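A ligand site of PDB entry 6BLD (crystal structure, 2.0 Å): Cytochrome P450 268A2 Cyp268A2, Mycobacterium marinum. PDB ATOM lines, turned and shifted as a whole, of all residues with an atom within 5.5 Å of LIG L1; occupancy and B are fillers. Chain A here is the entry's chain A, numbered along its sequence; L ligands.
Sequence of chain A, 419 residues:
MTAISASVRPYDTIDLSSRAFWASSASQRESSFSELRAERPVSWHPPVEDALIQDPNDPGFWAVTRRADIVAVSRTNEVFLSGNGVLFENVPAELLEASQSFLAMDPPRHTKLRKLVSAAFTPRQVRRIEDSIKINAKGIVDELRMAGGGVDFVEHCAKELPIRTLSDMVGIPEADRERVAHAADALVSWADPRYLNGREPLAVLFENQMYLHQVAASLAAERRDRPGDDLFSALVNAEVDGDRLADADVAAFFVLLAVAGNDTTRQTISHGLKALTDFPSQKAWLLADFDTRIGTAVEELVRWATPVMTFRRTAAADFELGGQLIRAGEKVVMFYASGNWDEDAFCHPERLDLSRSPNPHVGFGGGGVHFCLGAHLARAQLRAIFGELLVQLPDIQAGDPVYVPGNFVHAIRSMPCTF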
ATOM      1  N   LEU A  87     -30.424 -21.035  19.462  1.00  0.00           N
ATOM      2  CA  LEU A  87     -31.510 -21.511  20.308  1.00  0.00           C
ATOM      3  C   LEU A  87     -32.792 -20.737  20.033  1.00  0.00           C
ATOM      4  O   LEU A  87     -32.756 -19.528  19.757  1.00  0.00           O
ATOM      5  CB  LEU A  87     -31.131 -21.412  21.784  1.00  0.00           C
ATOM      6  CG  LEU A  87     -30.086 -22.420  22.262  1.00  0.00           C
ATOM      7  CD1 LEU A  87     -30.052 -22.486  23.790  1.00  0.00           C
ATOM      8  CD2 LEU A  87     -30.330 -23.801  21.670  1.00  0.00           C
ATOM      9  N   VAL A  91     -31.824 -16.916  25.631  1.00  0.00           N
ATOM     10  CA  VAL A  91     -31.063 -17.442  26.768  1.00  0.00           C
ATOM     11  C   VAL A  91     -29.965 -16.442  27.121  1.00  0.00           C
ATOM     12  O   VAL A  91     -29.357 -15.857  26.209  1.00  0.00           O
ATOM     13  CB  VAL A  91     -30.494 -18.830  26.453  1.00  0.00           C
ATOM     14  CG1 VAL A  91     -29.609 -19.344  27.590  1.00  0.00           C
ATOM     15  CG2 VAL A  91     -31.607 -19.816  26.141  1.00  0.00           C
ATOM     16  N   LEU A  95     -24.699 -17.985  29.744  1.00  0.00           N
ATOM     17  CA  LEU A  95     -25.034 -19.397  29.636  1.00  0.00           C
ATOM     18  C   LEU A  95     -24.786 -19.921  28.224  1.00  0.00           C
ATOM     19  O   LEU A  95     -24.369 -21.072  28.047  1.00  0.00           O
ATOM     20  CB  LEU A  95     -26.491 -19.627  30.044  1.00  0.00           C
ATOM     21  CG  LEU A  95     -26.818 -19.325  31.505  1.00  0.00           C
ATOM     22  CD1 LEU A  95     -28.330 -19.310  31.739  1.00  0.00           C
ATOM     23  CD2 LEU A  95     -26.134 -20.329  32.425  1.00  0.00           C
ATOM     24  N   SER A  99     -21.635 -22.890  26.655  1.00  0.00           N
ATOM     25  CA  SER A  99     -22.255 -24.158  26.240  1.00  0.00           C
ATOM     26  C   SER A  99     -22.343 -24.377  24.738  1.00  0.00           C
ATOM     27  O   SER A  99     -22.358 -25.529  24.316  1.00  0.00           O
ATOM     28  CB  SER A  99     -23.668 -24.256  26.825  1.00  0.00           C
ATOM     29  OG  SER A  99     -24.500 -23.222  26.318  1.00  0.00           O
ATOM     30  N   GLN A 100     -22.379 -23.329  23.907  1.00  0.00           N
ATOM     31  CA  GLN A 100     -22.713 -23.516  22.502  1.00  0.00           C
ATOM     32  C   GLN A 100     -21.527 -24.018  21.683  1.00  0.00           C
ATOM     33  O   GLN A 100     -21.710 -24.887  20.813  1.00  0.00           O
ATOM     34  CB  GLN A 100     -23.247 -22.211  21.912  1.00  0.00           C
ATOM     35  CG  GLN A 100     -24.535 -21.706  22.567  1.00  0.00           C
ATOM     36  CD  GLN A 100     -25.663 -22.721  22.488  1.00  0.00           C
ATOM     37  OE1 GLN A 100     -26.360 -22.827  21.477  1.00  0.00           O
ATOM     38  NE2 GLN A 100     -25.851 -23.476  23.571  1.00  0.00           N
ATOM     39  N   LEU A 103     -21.287 -24.981  17.670  1.00  0.00           N
ATOM     40  CA  LEU A 103     -22.666 -25.096  17.211  1.00  0.00           C
ATOM     41  C   LEU A 103     -23.232 -23.733  16.833  1.00  0.00           C
ATOM     42  O   LEU A 103     -23.918 -23.600  15.809  1.00  0.00           O
ATOM     43  CB  LEU A 103     -23.527 -25.766  18.283  1.00  0.00           C
ATOM     44  CG  LEU A 103     -25.029 -25.834  17.985  1.00  0.00           C
ATOM     45  CD1 LEU A 103     -25.327 -26.911  16.952  1.00  0.00           C
ATOM     46  CD2 LEU A 103     -25.813 -26.093  19.270  1.00  0.00           C
ATOM     47  N   LEU A 187     -29.518 -29.108  31.334  1.00  0.00           N
ATOM     48  CA  LEU A 187     -29.345 -27.921  30.505  1.00  0.00           C
ATOM     49  C   LEU A 187     -30.410 -27.773  29.425  1.00  0.00           C
ATOM     50  O   LEU A 187     -30.447 -26.731  28.763  1.00  0.00           O
ATOM     51  CB  LEU A 187     -27.949 -27.927  29.872  1.00  0.00           C
ATOM     52  CG  LEU A 187     -26.803 -27.847  30.879  1.00  0.00           C
ATOM     53  CD1 LEU A 187     -25.458 -27.766  30.184  1.00  0.00           C
ATOM     54  CD2 LEU A 187     -27.007 -26.667  31.812  1.00  0.00           C
ATOM     55  N   VAL A 188     -31.256 -28.778  29.232  1.00  0.00           N
ATOM     56  CA  VAL A 188     -32.367 -28.690  28.292  1.00  0.00           C
ATOM     57  C   VAL A 188     -33.713 -28.815  28.984  1.00  0.00           C
ATOM     58  O   VAL A 188     -34.744 -28.897  28.321  1.00  0.00           O
ATOM     59  CB  VAL A 188     -32.231 -29.730  27.168  1.00  0.00           C
ATOM     60  CG1 VAL A 188     -30.892 -29.571  26.447  1.00  0.00           C
ATOM     61  CG2 VAL A 188     -32.387 -31.136  27.721  1.00  0.00           C
ATOM     62  N   TRP A 190     -34.976 -26.582  31.392  1.00  0.00           N
ATOM     63  CA  TRP A 190     -35.215 -25.355  32.156  1.00  0.00           C
ATOM     64  C   TRP A 190     -36.685 -24.965  32.205  1.00  0.00           C
ATOM     65  O   TRP A 190     -37.049 -24.083  32.982  1.00  0.00           O
ATOM     66  CB  TRP A 190     -34.394 -24.210  31.567  1.00  0.00           C
ATOM     67  CG  TRP A 190     -34.821 -23.760  30.195  1.00  0.00           C
ATOM     68  CD1 TRP A 190     -35.849 -22.925  29.889  1.00  0.00           C
ATOM     69  CD2 TRP A 190     -34.211 -24.120  28.942  1.00  0.00           C
ATOM     70  NE1 TRP A 190     -35.930 -22.751  28.526  1.00  0.00           N
ATOM     71  CE2 TRP A 190     -34.933 -23.467  27.925  1.00  0.00           C
ATOM     72  CE3 TRP A 190     -33.132 -24.935  28.587  1.00  0.00           C
ATOM     73  CZ2 TRP A 190     -34.607 -23.612  26.580  1.00  0.00           C
ATOM     74  CZ3 TRP A 190     -32.809 -25.067  27.253  1.00  0.00           C
ATOM     75  CH2 TRP A 190     -33.543 -24.412  26.265  1.00  0.00           C
ATOM     76  N   LEU A 205     -29.364 -23.862  35.828  1.00  0.00           N
ATOM     77  CA  LEU A 205     -28.559 -23.978  34.625  1.00  0.00           C
ATOM     78  C   LEU A 205     -27.088 -23.665  34.903  1.00  0.00           C
ATOM     79  O   LEU A 205     -26.197 -24.358  34.424  1.00  0.00           O
ATOM     80  CB  LEU A 205     -29.113 -23.066  33.533  1.00  0.00           C
ATOM     81  CG  LEU A 205     -30.464 -23.452  32.934  1.00  0.00           C
ATOM     82  CD1 LEU A 205     -30.964 -22.381  31.976  1.00  0.00           C
ATOM     83  CD2 LEU A 205     -30.378 -24.806  32.229  1.00  0.00           C
ATOM     84  N   GLN A 209     -23.959 -26.189  34.523  1.00  0.00           N
ATOM     85  CA  GLN A 209     -22.892 -25.737  33.647  1.00  0.00           C
ATOM     86  C   GLN A 209     -21.584 -25.624  34.401  1.00  0.00           C
ATOM     87  O   GLN A 209     -20.516 -25.983  33.872  1.00  0.00           O
ATOM     88  CB  GLN A 209     -23.256 -24.392  33.019  1.00  0.00           C
ATOM     89  CG  GLN A 209     -24.088 -24.496  31.751  1.00  0.00           C
ATOM     90  CD  GLN A 209     -24.164 -23.182  31.011  1.00  0.00           C
ATOM     91  OE1 GLN A 209     -23.519 -22.207  31.386  1.00  0.00           O
ATOM     92  NE2 GLN A 209     -24.966 -23.143  29.947  1.00  0.00           N
ATOM     93  N   VAL A 255     -19.292 -29.050  27.160  1.00  0.00           N
ATOM     94  CA  VAL A 255     -20.726 -28.929  27.403  1.00  0.00           C
ATOM     95  C   VAL A 255     -21.517 -29.283  26.165  1.00  0.00           C
ATOM     96  O   VAL A 255     -22.468 -30.065  26.213  1.00  0.00           O
ATOM     97  CB  VAL A 255     -21.068 -27.507  27.898  1.00  0.00           C
ATOM     98  CG1 VAL A 255     -22.571 -27.357  28.086  1.00  0.00           C
ATOM     99  CG2 VAL A 255     -20.323 -27.201  29.187  1.00  0.00           C
ATOM    100  N   LEU A 256     -21.141 -28.714  25.018  1.00  0.00           N
ATOM    101  CA  LEU A 256     -21.796 -29.056  23.764  1.00  0.00           C
ATOM    102  C   LEU A 256     -21.770 -30.567  23.520  1.00  0.00           C
ATOM    103  O   LEU A 256     -22.807 -31.171  23.194  1.00  0.00           O
ATOM    104  CB  LEU A 256     -21.130 -28.322  22.610  1.00  0.00           C
ATOM    105  CG  LEU A 256     -21.521 -28.726  21.193  1.00  0.00           C
ATOM    106  CD1 LEU A 256     -23.028 -28.594  20.971  1.00  0.00           C
ATOM    107  CD2 LEU A 256     -20.738 -27.948  20.141  1.00  0.00           C
ATOM    108  N   VAL A 259     -24.057 -32.433  26.147  1.00  0.00           N
ATOM    109  CA  VAL A 259     -25.491 -32.253  25.976  1.00  0.00           C
ATOM    110  C   VAL A 259     -25.978 -32.951  24.706  1.00  0.00           C
ATOM    111  O   VAL A 259     -26.929 -33.736  24.741  1.00  0.00           O
ATOM    112  CB  VAL A 259     -25.856 -30.759  25.960  1.00  0.00           C
ATOM    113  CG1 VAL A 259     -27.326 -30.577  25.615  1.00  0.00           C
ATOM    114  CG2 VAL A 259     -25.540 -30.124  27.317  1.00  0.00           C
ATOM    115  N   ALA A 260     -25.325 -32.672  23.575  1.00  0.00           N
ATOM    116  CA  ALA A 260     -25.750 -33.278  22.324  1.00  0.00           C
ATOM    117  C   ALA A 260     -25.490 -34.785  22.304  1.00  0.00           C
ATOM    118  O   ALA A 260     -26.285 -35.537  21.713  1.00  0.00           O
ATOM    119  CB  ALA A 260     -25.043 -32.610  21.148  1.00  0.00           C
ATOM    120  N   THR A 264     -29.935 -36.275  23.212  1.00  0.00           N
ATOM    121  CA  THR A 264     -30.633 -36.659  21.984  1.00  0.00           C
ATOM    122  C   THR A 264     -30.835 -38.170  21.902  1.00  0.00           C
ATOM    123  O   THR A 264     -31.960 -38.648  21.695  1.00  0.00           O
ATOM    124  CB  THR A 264     -29.849 -36.168  20.768  1.00  0.00           C
ATOM    125  OG1 THR A 264     -28.507 -36.677  20.825  1.00  0.00           O
ATOM    126  CG2 THR A 264     -29.804 -34.649  20.745  1.00  0.00           C
ATOM    127  N   VAL A 308     -34.486 -33.246  18.890  1.00  0.00           N
ATOM    128  CA  VAL A 308     -34.246 -31.818  18.736  1.00  0.00           C
ATOM    129  C   VAL A 308     -35.418 -31.239  17.950  1.00  0.00           C
ATOM    130  O   VAL A 308     -35.569 -31.519  16.757  1.00  0.00           O
ATOM    131  CB  VAL A 308     -32.908 -31.534  18.036  1.00  0.00           C
ATOM    132  CG1 VAL A 308     -32.640 -30.040  17.989  1.00  0.00           C
ATOM    133  CG2 VAL A 308     -31.778 -32.266  18.736  1.00  0.00           C
ATOM    134  N   PHE A 311     -34.171 -25.393  16.134  1.00  0.00           N
ATOM    135  CA  PHE A 311     -32.900 -24.693  16.036  1.00  0.00           C
ATOM    136  C   PHE A 311     -33.155 -23.473  15.164  1.00  0.00           C
ATOM    137  O   PHE A 311     -33.973 -23.514  14.252  1.00  0.00           O
ATOM    138  CB  PHE A 311     -31.779 -25.556  15.451  1.00  0.00           C
ATOM    139  CG  PHE A 311     -30.913 -26.231  16.482  1.00  0.00           C
ATOM    140  CD1 PHE A 311     -30.524 -25.552  17.629  1.00  0.00           C
ATOM    141  CD2 PHE A 311     -30.498 -27.534  16.305  1.00  0.00           C
ATOM    142  CE1 PHE A 311     -29.730 -26.174  18.577  1.00  0.00           C
ATOM    143  CE2 PHE A 311     -29.702 -28.165  17.256  1.00  0.00           C
ATOM    144  CZ  PHE A 311     -29.316 -27.480  18.387  1.00  0.00           C
ATOM    145  N   PHE A 408     -37.326 -26.946  23.143  1.00  0.00           N
ATOM    146  CA  PHE A 408     -36.061 -27.320  22.530  1.00  0.00           C
ATOM    147  C   PHE A 408     -35.955 -28.823  22.289  1.00  0.00           C
ATOM    148  O   PHE A 408     -35.757 -29.239  21.144  1.00  0.00           O
ATOM    149  CB  PHE A 408     -34.890 -26.837  23.404  1.00  0.00           C
ATOM    150  CG  PHE A 408     -33.530 -27.088  22.802  1.00  0.00           C
ATOM    151  CD1 PHE A 408     -33.343 -27.093  21.428  1.00  0.00           C
ATOM    152  CD2 PHE A 408     -32.435 -27.327  23.625  1.00  0.00           C
ATOM    153  CE1 PHE A 408     -32.095 -27.328  20.877  1.00  0.00           C
ATOM    154  CE2 PHE A 408     -31.179 -27.558  23.081  1.00  0.00           C
ATOM    155  CZ  PHE A 408     -31.009 -27.559  21.707  1.00  0.00           C
ATOM    156  N   VAL A 409     -36.089 -29.646  23.320  1.00  0.00           N
ATOM    157  CA  VAL A 409     -35.897 -31.086  23.221  1.00  0.00           C
ATOM    158  C   VAL A 409     -37.213 -31.792  23.505  1.00  0.00           C
ATOM    159  O   VAL A 409     -37.895 -31.466  24.485  1.00  0.00           O
ATOM    160  CB  VAL A 409     -34.789 -31.575  24.169  1.00  0.00           C
ATOM    161  CG1 VAL A 409     -34.769 -33.090  24.247  1.00  0.00           C
ATOM    162  CG2 VAL A 409     -33.435 -31.044  23.722  1.00  0.00           C
HETATM  163  C1  LIG L   1     -27.222 -25.815  25.978  1.00  0.00           C
HETATM  164  C2  LIG L   1     -28.922 -23.804  28.762  1.00  0.00           C
HETATM  165  C3  LIG L   1     -27.822 -30.853  19.072  1.00  0.00           C
HETATM  166  C4  LIG L   1     -27.876 -30.362  20.513  1.00  0.00           C
HETATM  167  C5  LIG L   1     -26.991 -29.486  20.940  1.00  0.00           C
HETATM  168  C6  LIG L   1     -28.953 -30.897  21.467  1.00  0.00           C
HETATM  169  C7  LIG L   1     -27.012 -28.982  22.385  1.00  0.00           C
HETATM  170  C8  LIG L   1     -26.913 -27.455  22.459  1.00  0.00           C
HETATM  171  C9  LIG L   1     -26.600 -26.950  23.869  1.00  0.00           C
HETATM  172  C10 LIG L   1     -27.525 -26.329  24.563  1.00  0.00           C
HETATM  173  C11 LIG L   1     -25.213 -27.180  24.469  1.00  0.00           C
HETATM  174  C12 LIG L   1     -28.067 -24.975  26.559  1.00  0.00           C
HETATM  175  C13 LIG L   1     -27.785 -24.451  27.958  1.00  0.00           C
HETATM  176  O1  LIG L   1     -26.707 -24.538  28.425  1.00  0.00           O
HETATM  177  C1  LG2 L   2     -25.460 -31.139  15.778  1.00  0.00           C
HETATM  178  C2  LG2 L   2     -22.947 -34.161  18.625  1.00  0.00           C
HETATM  179  C3  LG2 L   2     -26.605 -37.343  18.490  1.00  0.00           C
HETATM  180  C4  LG2 L   2     -29.374 -33.938  16.398  1.00  0.00           C
HETATM  181  C5  LG2 L   2     -24.458 -31.683  16.554  1.00  0.00           C
HETATM  182  C6  LG2 L   2     -23.165 -31.075  16.833  1.00  0.00           C
HETATM  183  C7  LG2 L   2     -22.474 -31.900  17.616  1.00  0.00           C
HETATM  184  C8  LG2 L   2     -23.294 -33.079  17.863  1.00  0.00           C
HETATM  185  C9  LG2 L   2     -21.051 -31.663  18.160  1.00  0.00           C
HETATM  186  C10 LG2 L   2     -22.685 -29.709  16.314  1.00  0.00           C
HETATM  187  C11 LG2 L   2     -22.139 -29.888  14.903  1.00  0.00           C
HETATM  188  C12 LG2 L   2     -21.833 -28.552  14.288  1.00  0.00           C
HETATM  189  O1  LG2 L   2     -21.065 -28.506  13.288  1.00  0.00           O
HETATM  190  O2  LG2 L   2     -22.344 -27.523  14.796  1.00  0.00           O
HETATM  191  C13 LG2 L   2     -23.686 -35.320  18.785  1.00  0.00           C
HETATM  192  C14 LG2 L   2     -23.223 -36.536  19.400  1.00  0.00           C
HETATM  193  C15 LG2 L   2     -24.205 -37.432  19.375  1.00  0.00           C
HETATM  194  C16 LG2 L   2     -25.361 -36.803  18.737  1.00  0.00           C
HETATM  195  C17 LG2 L   2     -21.816 -36.783  19.988  1.00  0.00           C
HETATM  196  C18 LG2 L   2     -24.060 -38.854  19.957  1.00  0.00           C
HETATM  197  C19 LG2 L   2     -25.002 -39.792  19.831  1.00  0.00           C
HETATM  198  C20 LG2 L   2     -27.683 -36.708  17.906  1.00  0.00           C
HETATM  199  C21 LG2 L   2     -28.988 -37.276  17.632  1.00  0.00           C
HETATM  200  C22 LG2 L   2     -29.750 -36.319  17.061  1.00  0.00           C
HETATM  201  C23 LG2 L   2     -28.942 -35.125  16.949  1.00  0.00           C
HETATM  202  C24 LG2 L   2     -29.375 -38.732  17.988  1.00  0.00           C
HETATM  203  C25 LG2 L   2     -31.206 -36.375  16.554  1.00  0.00           C
HETATM  204  C26 LG2 L   2     -31.908 -37.500  16.420  1.00  0.00           C
HETATM  205  C27 LG2 L   2     -28.563 -32.888  16.029  1.00  0.00           C
HETATM  206  C28 LG2 L   2     -28.986 -31.688  15.328  1.00  0.00           C
HETATM  207  C29 LG2 L   2     -27.906 -30.911  15.153  1.00  0.00           C
HETATM  208  C30 LG2 L   2     -26.759 -31.598  15.740  1.00  0.00           C
HETATM  209  C31 LG2 L   2     -30.428 -31.380  14.872  1.00  0.00           C
HETATM  210  C32 LG2 L   2     -27.876 -29.540  14.453  1.00  0.00           C
HETATM  211  C33 LG2 L   2     -27.870 -29.750  12.939  1.00  0.00           C
HETATM  212  C34 LG2 L   2     -27.902 -28.429  12.209  1.00  0.00           C
HETATM  213  O3  LG2 L   2     -27.958 -28.449  10.958  1.00  0.00           O
HETATM  214  O4  LG2 L   2     -27.864 -27.374  12.880  1.00  0.00           O
HETATM  215  N1  LG2 L   2     -24.491 -32.905  17.197  1.00  0.00           N
HETATM  216  N2  LG2 L   2     -24.987 -35.514  18.385  1.00  0.00           N
HETATM  217  N3  LG2 L   2     -27.695 -35.390  17.468  1.00  0.00           N
HETATM  218  N4  LG2 L   2     -27.213 -32.789  16.267  1.00  0.00           N
HETATM  219 FE1  LG2 L   2     -26.045 -34.244  17.117  1.00  0.00          FE
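Gln 100 touches LIG L1.
Leu 103 touches LIG L1 (CD2 to C8, 3.6 Å).
O of Leu 187 touches C2 of LIG L1, 3.3 Å away.
Leu 205 touches LIG L1.
CA of Leu 256 touches C11 of LIG L1, at 3.96 Å.
CG1 of Val 259 touches C7 of LIG L1, at 3.6 Å.
CB of Ala 260 touches C4 of LIG L1, 3.7 Å away.
Thr 264 touches LIG L1.
Phe 311 touches LIG L1 (CE2 to C3, 3.7 Å).
Phe 408 touches LIG L1 (CZ to C6, 3.9 Å).
12 residues have an atom within 4 Å of LIG L1: Ser 99, Gln 100, Leu 103, Leu 187, Leu 205, Gln 209, Leu 256, Val 259, Ala 260, Thr 264, Phe 311 and Phe 408.
Along chain A the residues within 4 Å of LIG L1 span positions 99 to 408.
NE2 of Gln 209 is in hydrogen-bond range of O of Leu 95, 2.9 Å away.
OG of Ser 99 sits at hydrogen-bond distance from NE2 of Gln 100 (3.1 Å).
The backbone carbonyl oxygen of Ser 99 is in hydrogen-bond range of the backbone NH of Leu 256 (3.5 Å).
OG of Ser 99 lies within hydrogen-bond range of O of Leu 95.
OG1 of Thr 264 is in hydrogen-bond range of O of Ala 260 (2.7 Å).
The side-chain amide nitrogen (NE2) of Gln 209 is in hydrogen-bond range of an oxygen (O1) of LIG L1, at 2.7 Å.
O1 of LIG L1 lies within hydrogen-bond range of OG of Ser 99, at 3.3 Å.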
